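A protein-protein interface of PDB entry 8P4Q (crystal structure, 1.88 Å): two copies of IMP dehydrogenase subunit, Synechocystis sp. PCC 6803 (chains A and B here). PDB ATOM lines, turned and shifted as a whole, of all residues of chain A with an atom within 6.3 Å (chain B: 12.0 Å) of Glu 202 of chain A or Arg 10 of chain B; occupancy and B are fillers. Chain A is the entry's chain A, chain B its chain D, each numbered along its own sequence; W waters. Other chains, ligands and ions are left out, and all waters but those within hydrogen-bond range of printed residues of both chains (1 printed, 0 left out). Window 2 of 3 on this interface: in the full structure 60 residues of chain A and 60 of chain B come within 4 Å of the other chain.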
ATOM      1  N   GLY A   1       5.140 -14.122   6.240  1.00  0.00           N
ATOM      2  CA  GLY A   1       4.179 -14.961   6.998  1.00  0.00           C
ATOM      3  C   GLY A   1       3.683 -14.272   8.245  1.00  0.00           C
ATOM      4  O   GLY A   1       4.332 -13.371   8.784  1.00  0.00           O
ATOM      5  N   THR A 200       6.547  -2.861  10.174  1.00  0.00           N
ATOM      6  CA  THR A 200       6.521  -4.226  10.685  1.00  0.00           C
ATOM      7  C   THR A 200       7.354  -4.377  11.953  1.00  0.00           C
ATOM      8  O   THR A 200       8.360  -3.689  12.155  1.00  0.00           O
ATOM      9  CB  THR A 200       7.025  -5.242   9.638  1.00  0.00           C
ATOM     10  OG1 THR A 200       8.385  -4.942   9.300  1.00  0.00           O
ATOM     11  CG2 THR A 200       6.157  -5.219   8.392  1.00  0.00           C
ATOM     12  N   TYR A 201       6.915  -5.309  12.804  1.00  0.00           N
ATOM     13  CA  TYR A 201       7.685  -5.700  13.981  1.00  0.00           C
ATOM     14  C   TYR A 201       9.110  -6.083  13.598  1.00  0.00           C
ATOM     15  O   TYR A 201      10.078  -5.632  14.220  1.00  0.00           O
ATOM     16  CB  TYR A 201       6.972  -6.867  14.681  1.00  0.00           C
ATOM     17  CG  TYR A 201       7.723  -7.480  15.839  1.00  0.00           C
ATOM     18  CD1 TYR A 201       8.749  -8.392  15.624  1.00  0.00           C
ATOM     19  CD2 TYR A 201       7.405  -7.153  17.147  1.00  0.00           C
ATOM     20  CE1 TYR A 201       9.454  -8.940  16.677  1.00  0.00           C
ATOM     21  CE2 TYR A 201       8.093  -7.715  18.211  1.00  0.00           C
ATOM     22  CZ  TYR A 201       9.113  -8.608  17.966  1.00  0.00           C
ATOM     23  OH  TYR A 201       9.802  -9.161  19.012  1.00  0.00           O
ATOM     24  N   GLU A 202       9.256  -6.912  12.565  1.00  0.00           N
ATOM     25  CA  GLU A 202      10.561  -7.481  12.243  1.00  0.00           C
ATOM     26  C   GLU A 202      11.568  -6.397  11.883  1.00  0.00           C
ATOM     27  O   GLU A 202      12.712  -6.417  12.352  1.00  0.00           O
ATOM     28  CB  GLU A 202      10.424  -8.488  11.104  1.00  0.00           C
ATOM     29  CG  GLU A 202       9.740  -9.794  11.479  1.00  0.00           C
ATOM     30  CD  GLU A 202       8.233  -9.663  11.668  1.00  0.00           C
ATOM     31  OE1 GLU A 202       7.634  -8.675  11.204  1.00  0.00           O
ATOM     32  OE2 GLU A 202       7.640 -10.565  12.280  1.00  0.00           O
ATOM     33  N   VAL A 203      11.169  -5.451  11.034  1.00  0.00           N
ATOM     34  CA  VAL A 203      12.098  -4.416  10.596  1.00  0.00           C
ATOM     35  C   VAL A 203      12.388  -3.444  11.734  1.00  0.00           C
ATOM     36  O   VAL A 203      13.546  -3.095  11.995  1.00  0.00           O
ATOM     37  CB  VAL A 203      11.548  -3.684   9.362  1.00  0.00           C
ATOM     38  CG1 VAL A 203      12.411  -2.470   9.062  1.00  0.00           C
ATOM     39  CG2 VAL A 203      11.495  -4.624   8.179  1.00  0.00           C
ATOM     40  N   SER A 204      11.343  -2.982  12.425  1.00  0.00           N
ATOM     41  CA  SER A 204      11.559  -2.031  13.510  1.00  0.00           C
ATOM     42  C   SER A 204      12.487  -2.611  14.571  1.00  0.00           C
ATOM     43  O   SER A 204      13.355  -1.905  15.089  1.00  0.00           O
ATOM     44  CB  SER A 204      10.226  -1.602  14.127  1.00  0.00           C
ATOM     45  OG  SER A 204       9.463  -2.717  14.548  1.00  0.00           O
ATOM     46  N   LEU A 205      12.335  -3.897  14.897  1.00  0.00           N
ATOM     47  CA  LEU A 205      13.230  -4.506  15.878  1.00  0.00           C
ATOM     48  C   LEU A 205      14.682  -4.475  15.406  1.00  0.00           C
ATOM     49  O   LEU A 205      15.597  -4.246  16.206  1.00  0.00           O
ATOM     50  CB  LEU A 205      12.800  -5.945  16.160  1.00  0.00           C
ATOM     51  CG  LEU A 205      13.639  -6.716  17.182  1.00  0.00           C
ATOM     52  CD1 LEU A 205      13.730  -5.987  18.514  1.00  0.00           C
ATOM     53  CD2 LEU A 205      13.090  -8.128  17.379  1.00  0.00           C
ATOM     54  N   GLU A 206      14.916  -4.736  14.117  1.00  0.00           N
ATOM     55  CA  GLU A 206      16.283  -4.716  13.602  1.00  0.00           C
ATOM     56  C   GLU A 206      16.848  -3.300  13.567  1.00  0.00           C
ATOM     57  O   GLU A 206      18.050  -3.099  13.779  1.00  0.00           O
ATOM     58  CB  GLU A 206      16.329  -5.356  12.214  1.00  0.00           C
ATOM     59  CG  GLU A 206      16.123  -6.871  12.223  1.00  0.00           C
ATOM     60  CD  GLU A 206      16.956  -7.585  13.290  1.00  0.00           C
ATOM     61  OE1 GLU A 206      18.202  -7.541  13.186  1.00  0.00           O
ATOM     62  OE2 GLU A 206      16.370  -8.174  14.234  1.00  0.00           O
ATOM     63  N   LEU A 207      16.005  -2.306  13.273  1.00  0.00           N
ATOM     64  CA  LEU A 207      16.454  -0.916  13.333  1.00  0.00           C
ATOM     65  C   LEU A 207      16.873  -0.540  14.751  1.00  0.00           C
ATOM     66  O   LEU A 207      17.878   0.149  14.960  1.00  0.00           O
ATOM     67  CB  LEU A 207      15.345   0.006  12.825  1.00  0.00           C
ATOM     68  CG  LEU A 207      14.962  -0.131  11.349  1.00  0.00           C
ATOM     69  CD1 LEU A 207      13.718   0.717  11.049  1.00  0.00           C
ATOM     70  CD2 LEU A 207      16.116   0.261  10.445  1.00  0.00           C
ATOM     71  N   THR A 239      -2.346  -0.471  13.067  1.00  0.00           N
ATOM     72  CA  THR A 239      -1.693  -1.776  13.044  1.00  0.00           C
ATOM     73  C   THR A 239      -0.178  -1.630  13.003  1.00  0.00           C
ATOM     74  O   THR A 239       0.538  -2.303  13.752  1.00  0.00           O
ATOM     75  CB  THR A 239      -2.194  -2.588  11.851  1.00  0.00           C
ATOM     76  OG1 THR A 239      -3.593  -2.853  12.011  1.00  0.00           O
ATOM     77  CG2 THR A 239      -1.425  -3.896  11.730  1.00  0.00           C
ATOM     78  N   ALA A 242       1.192  -0.423  16.429  1.00  0.00           N
ATOM     79  CA  ALA A 242       1.149  -1.451  17.464  1.00  0.00           C
ATOM     80  C   ALA A 242       2.241  -2.497  17.259  1.00  0.00           C
ATOM     81  O   ALA A 242       2.909  -2.898  18.218  1.00  0.00           O
ATOM     82  CB  ALA A 242      -0.227  -2.113  17.495  1.00  0.00           C
ATOM     83  N   ASP A 243       2.432  -2.956  16.017  1.00  0.00           N
ATOM     84  CA  ASP A 243       3.480  -3.940  15.746  1.00  0.00           C
ATOM     85  C   ASP A 243       4.858  -3.398  16.104  1.00  0.00           C
ATOM     86  O   ASP A 243       5.690  -4.119  16.670  1.00  0.00           O
ATOM     87  CB  ASP A 243       3.451  -4.359  14.272  1.00  0.00           C
ATOM     88  CG  ASP A 243       2.323  -5.325  13.953  1.00  0.00           C
ATOM     89  OD1 ASP A 243       1.642  -5.788  14.889  1.00  0.00           O
ATOM     90  OD2 ASP A 243       2.105  -5.623  12.760  1.00  0.00           O
ATOM     91  N   ALA A 245       5.489  -0.894  18.203  1.00  0.00           N
ATOM     92  CA  ALA A 245       5.553  -0.714  19.649  1.00  0.00           C
ATOM     93  C   ALA A 245       5.875  -2.025  20.358  1.00  0.00           C
ATOM     94  O   ALA A 245       6.572  -2.025  21.377  1.00  0.00           O
ATOM     95  CB  ALA A 245       4.241  -0.140  20.175  1.00  0.00           C
ATOM     96  N   ALA A 246       5.365  -3.147  19.843  1.00  0.00           N
ATOM     97  CA  ALA A 246       5.704  -4.447  20.416  1.00  0.00           C
ATOM     98  C   ALA A 246       7.193  -4.738  20.267  1.00  0.00           C
ATOM     99  O   ALA A 246       7.822  -5.289  21.177  1.00  0.00           O
ATOM    100  CB  ALA A 246       4.869  -5.545  19.760  1.00  0.00           C
ATOM    101  N   ALA A 247       7.775  -4.369  19.124  1.00  0.00           N
ATOM    102  CA  ALA A 247       9.215  -4.514  18.949  1.00  0.00           C
ATOM    103  C   ALA A 247       9.973  -3.674  19.967  1.00  0.00           C
ATOM    104  O   ALA A 247      10.966  -4.130  20.547  1.00  0.00           O
ATOM    105  CB  ALA A 247       9.609  -4.118  17.525  1.00  0.00           C
ATOM    106  N   ASP A 250       9.885  -5.472  23.287  1.00  0.00           N
ATOM    107  CA  ASP A 250      10.773  -6.633  23.311  1.00  0.00           C
ATOM    108  C   ASP A 250      12.240  -6.208  23.335  1.00  0.00           C
ATOM    109  O   ASP A 250      13.057  -6.818  24.034  1.00  0.00           O
ATOM    110  CB  ASP A 250      10.489  -7.544  22.116  1.00  0.00           C
ATOM    111  CG  ASP A 250       9.203  -8.333  22.278  1.00  0.00           C
ATOM    112  OD1 ASP A 250       8.731  -8.469  23.425  1.00  0.00           O
ATOM    113  OD2 ASP A 250       8.664  -8.821  21.261  1.00  0.00           O
ATOM    114  N   ASN B   5     -11.267  -9.541  21.837  1.00  0.00           N
ATOM    115  CA  ASN B   5      -9.952  -8.987  21.557  1.00  0.00           C
ATOM    116  C   ASN B   5      -9.581  -9.205  20.086  1.00  0.00           C
ATOM    117  O   ASN B   5      -8.713 -10.011  19.743  1.00  0.00           O
ATOM    118  CB  ASN B   5      -8.894  -9.589  22.485  1.00  0.00           C
ATOM    119  N   ILE B   6     -10.251  -8.460  19.202  1.00  0.00           N
ATOM    120  CA  ILE B   6      -9.762  -8.319  17.837  1.00  0.00           C
ATOM    121  C   ILE B   6      -8.363  -7.729  17.872  1.00  0.00           C
ATOM    122  O   ILE B   6      -8.068  -6.834  18.671  1.00  0.00           O
ATOM    123  CB  ILE B   6     -10.704  -7.430  17.007  1.00  0.00           C
ATOM    124  CG1 ILE B   6     -12.025  -8.143  16.726  1.00  0.00           C
ATOM    125  CG2 ILE B   6     -10.021  -7.010  15.709  1.00  0.00           C
ATOM    126  CD1 ILE B   6     -13.071  -7.232  16.112  1.00  0.00           C
ATOM    127  N   THR B   7      -7.496  -8.196  16.979  1.00  0.00           N
ATOM    128  CA  THR B   7      -6.107  -7.751  16.975  1.00  0.00           C
ATOM    129  C   THR B   7      -5.931  -6.528  16.074  1.00  0.00           C
ATOM    130  O   THR B   7      -6.188  -6.593  14.867  1.00  0.00           O
ATOM    131  CB  THR B   7      -5.173  -8.880  16.529  1.00  0.00           C
ATOM    132  OG1 THR B   7      -5.285  -9.994  17.425  1.00  0.00           O
ATOM    133  CG2 THR B   7      -3.721  -8.394  16.507  1.00  0.00           C
ATOM    134  N   ILE B   8      -5.494  -5.416  16.668  1.00  0.00           N
ATOM    135  CA  ILE B   8      -5.010  -4.287  15.882  1.00  0.00           C
ATOM    136  C   ILE B   8      -3.573  -4.540  15.450  1.00  0.00           C
ATOM    137  O   ILE B   8      -3.231  -4.444  14.266  1.00  0.00           O
ATOM    138  CB  ILE B   8      -5.148  -2.981  16.686  1.00  0.00           C
ATOM    139  CG1 ILE B   8      -6.636  -2.615  16.775  1.00  0.00           C
ATOM    140  CG2 ILE B   8      -4.277  -1.894  16.077  1.00  0.00           C
ATOM    141  CD1 ILE B   8      -6.924  -1.463  17.673  1.00  0.00           C
ATOM    142  N   GLY B   9      -2.724  -4.906  16.401  1.00  0.00           N
ATOM    143  CA  GLY B   9      -1.373  -5.344  16.114  1.00  0.00           C
ATOM    144  C   GLY B   9      -0.886  -6.154  17.293  1.00  0.00           C
ATOM    145  O   GLY B   9      -1.622  -6.399  18.249  1.00  0.00           O
ATOM    146  N   ARG B  10       0.371  -6.576  17.217  1.00  0.00           N
ATOM    147  CA  ARG B  10       0.967  -7.296  18.333  1.00  0.00           C
ATOM    148  C   ARG B  10       0.826  -6.477  19.609  1.00  0.00           C
ATOM    149  O   ARG B  10       1.211  -5.305  19.655  1.00  0.00           O
ATOM    150  CB  ARG B  10       2.438  -7.600  18.037  1.00  0.00           C
ATOM    151  CG  ARG B  10       2.612  -8.530  16.842  1.00  0.00           C
ATOM    152  CD  ARG B  10       4.070  -8.757  16.478  1.00  0.00           C
ATOM    153  NE  ARG B  10       4.749  -9.582  17.470  1.00  0.00           N
ATOM    154  CZ  ARG B  10       5.752 -10.406  17.197  1.00  0.00           C
ATOM    155  NH1 ARG B  10       6.226 -10.536  15.970  1.00  0.00           N
ATOM    156  NH2 ARG B  10       6.294 -11.113  18.185  1.00  0.00           N
ATOM    157  N   GLY B  11       0.224  -7.085  20.625  1.00  0.00           N
ATOM    158  CA  GLY B  11       0.075  -6.444  21.917  1.00  0.00           C
ATOM    159  C   GLY B  11      -0.972  -5.361  22.014  1.00  0.00           C
ATOM    160  O   GLY B  11      -1.034  -4.680  23.042  1.00  0.00           O
ATOM    161  N   LYS B  12      -1.808  -5.176  20.990  1.00  0.00           N
ATOM    162  CA  LYS B  12      -2.888  -4.196  21.048  1.00  0.00           C
ATOM    163  C   LYS B  12      -4.143  -4.805  20.451  1.00  0.00           C
ATOM    164  O   LYS B  12      -4.163  -5.162  19.270  1.00  0.00           O
ATOM    165  CB  LYS B  12      -2.523  -2.907  20.308  1.00  0.00           C
ATOM    166  CG  LYS B  12      -3.476  -1.759  20.599  1.00  0.00           C
ATOM    167  CD  LYS B  12      -3.257  -1.189  21.998  1.00  0.00           C
ATOM    168  CE  LYS B  12      -4.403  -0.269  22.405  1.00  0.00           C
ATOM    169  NZ  LYS B  12      -4.180   0.376  23.732  1.00  0.00           N
ATOM    170  N   THR B  13      -5.185  -4.920  21.267  1.00  0.00           N
ATOM    171  CA  THR B  13      -6.451  -5.505  20.860  1.00  0.00           C
ATOM    172  C   THR B  13      -7.549  -4.453  20.929  1.00  0.00           C
ATOM    173  O   THR B  13      -7.364  -3.353  21.455  1.00  0.00           O
ATOM    174  CB  THR B  13      -6.816  -6.711  21.737  1.00  0.00           C
ATOM    175  OG1 THR B  13      -6.942  -6.292  23.101  1.00  0.00           O
ATOM    176  CG2 THR B  13      -5.771  -7.811  21.631  1.00  0.00           C
ATOM    177  N   ALA B  14      -8.708  -4.821  20.401  1.00  0.00           N
ATOM    178  CA  ALA B  14      -9.870  -3.947  20.383  1.00  0.00           C
ATOM    179  C   ALA B  14     -11.117  -4.815  20.305  1.00  0.00           C
ATOM    180  O   ALA B  14     -11.043  -6.016  20.034  1.00  0.00           O
ATOM    181  CB  ALA B  14      -9.801  -2.965  19.210  1.00  0.00           C
HETATM  182  O   HOH W   1       1.886  -3.156  20.856  1.00  0.00           O
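OD1 of Asp 243 of chain A lies within hydrogen-bond range of N of Arg 10 of chain B, 2.8 Å away. The backbone carbonyl oxygen (O) of Ile 8 of chain B lies within hydrogen-bond range of the side-chain hydroxyl (OG1) of Thr 239 of chain A, at 2.8 Å. OE2 of Glu 202 of chain A is in salt-bridge range of NH1 of Arg 10 of chain B, 3.95 Å away. O of Ala 242 of chain A lies close to O of Arg 10 of chain B (3.3 Å).
The side-chain hydroxyl (OG) of Ser 204 of chain A sits at hydrogen-bond distance from the backbone carbonyl oxygen (O) of Tyr 201 of chain A. OD2 of Asp 250 of chain A is in hydrogen-bond range of OH of Tyr 201 of chain A (2.5 Å).
Among the printed residues, pairs that only touch across the chains: Asp 243 of chain A with Gly 9 of chain B (3.3 Å), Tyr 201 of chain A with Arg 10 of chain B (3.3 Å), Ala 246 of chain A with Arg 10 of chain B (3.6 Å), Ala 242 of chain A with Gly 9 of chain B (3.7 Å) and Ala 242 of chain A with Lys 12 of chain B (3.7 Å).
No residue of chain B comes within 4 Å of Gly 1 of chain A. Of chain B, only Arg 10 (3.3 Å) comes within 4 Å of Tyr 201 of chain A. Of chain B, only Arg 10 (3.95 Å) comes within 4 Å of Glu 202 of chain A. Ser 204 of chain A touches none of the printed residues of chain B. Thr 239 of chain A touches just one residue of chain B: Ile 8 (2.8 Å). Of chain B, only Gly 9 (3.3 Å) and Arg 10 (2.8 Å) come within 4 Å of Asp 243 of chain A. Thr 7 of chain B touches none of the printed residues of chain A. Of the printed residues of chain A, Ile 8 of chain B touches Thr 239. Printed residues of chain A within 4 Å of Gly 9 of chain B: Ala 242 and Asp 243. Of chain A, only Tyr 201, Glu 202, Ala 242, Asp 243 and Ala 246 come within 4 Å of Arg 10 of chain B. Gly 11 of chain B touches none of the printed residues of chain A. Printed residues of chain A within 4 Å of Lys 12 of chain B: Ala 242. The nearest residue of chain B that does not touch Glu 202 of chain A is Gly 9 of chain B (10.8 Å).
Hydrophobic or aromatic side chains of chain B that line the printed part of chain A: Ile 8. Of the 16 printed residues of chain A, 6 touch a printed residue of chain B. Along chain A the printed residues that touch a printed residue of chain B span positions 201 to 246. Among the printed residues, Asp or Glu carboxylates within 4 Å of a Lys or Arg side-chain nitrogen of the other chain: Glu 202 of chain A with Arg 10 of chain B.
No position is printed for both chains.
Water W1 lies within hydrogen-bond range of O of Arg 10 of chain B (2.6 Å) and O of Ala 242 of chain A (2.8 Å).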
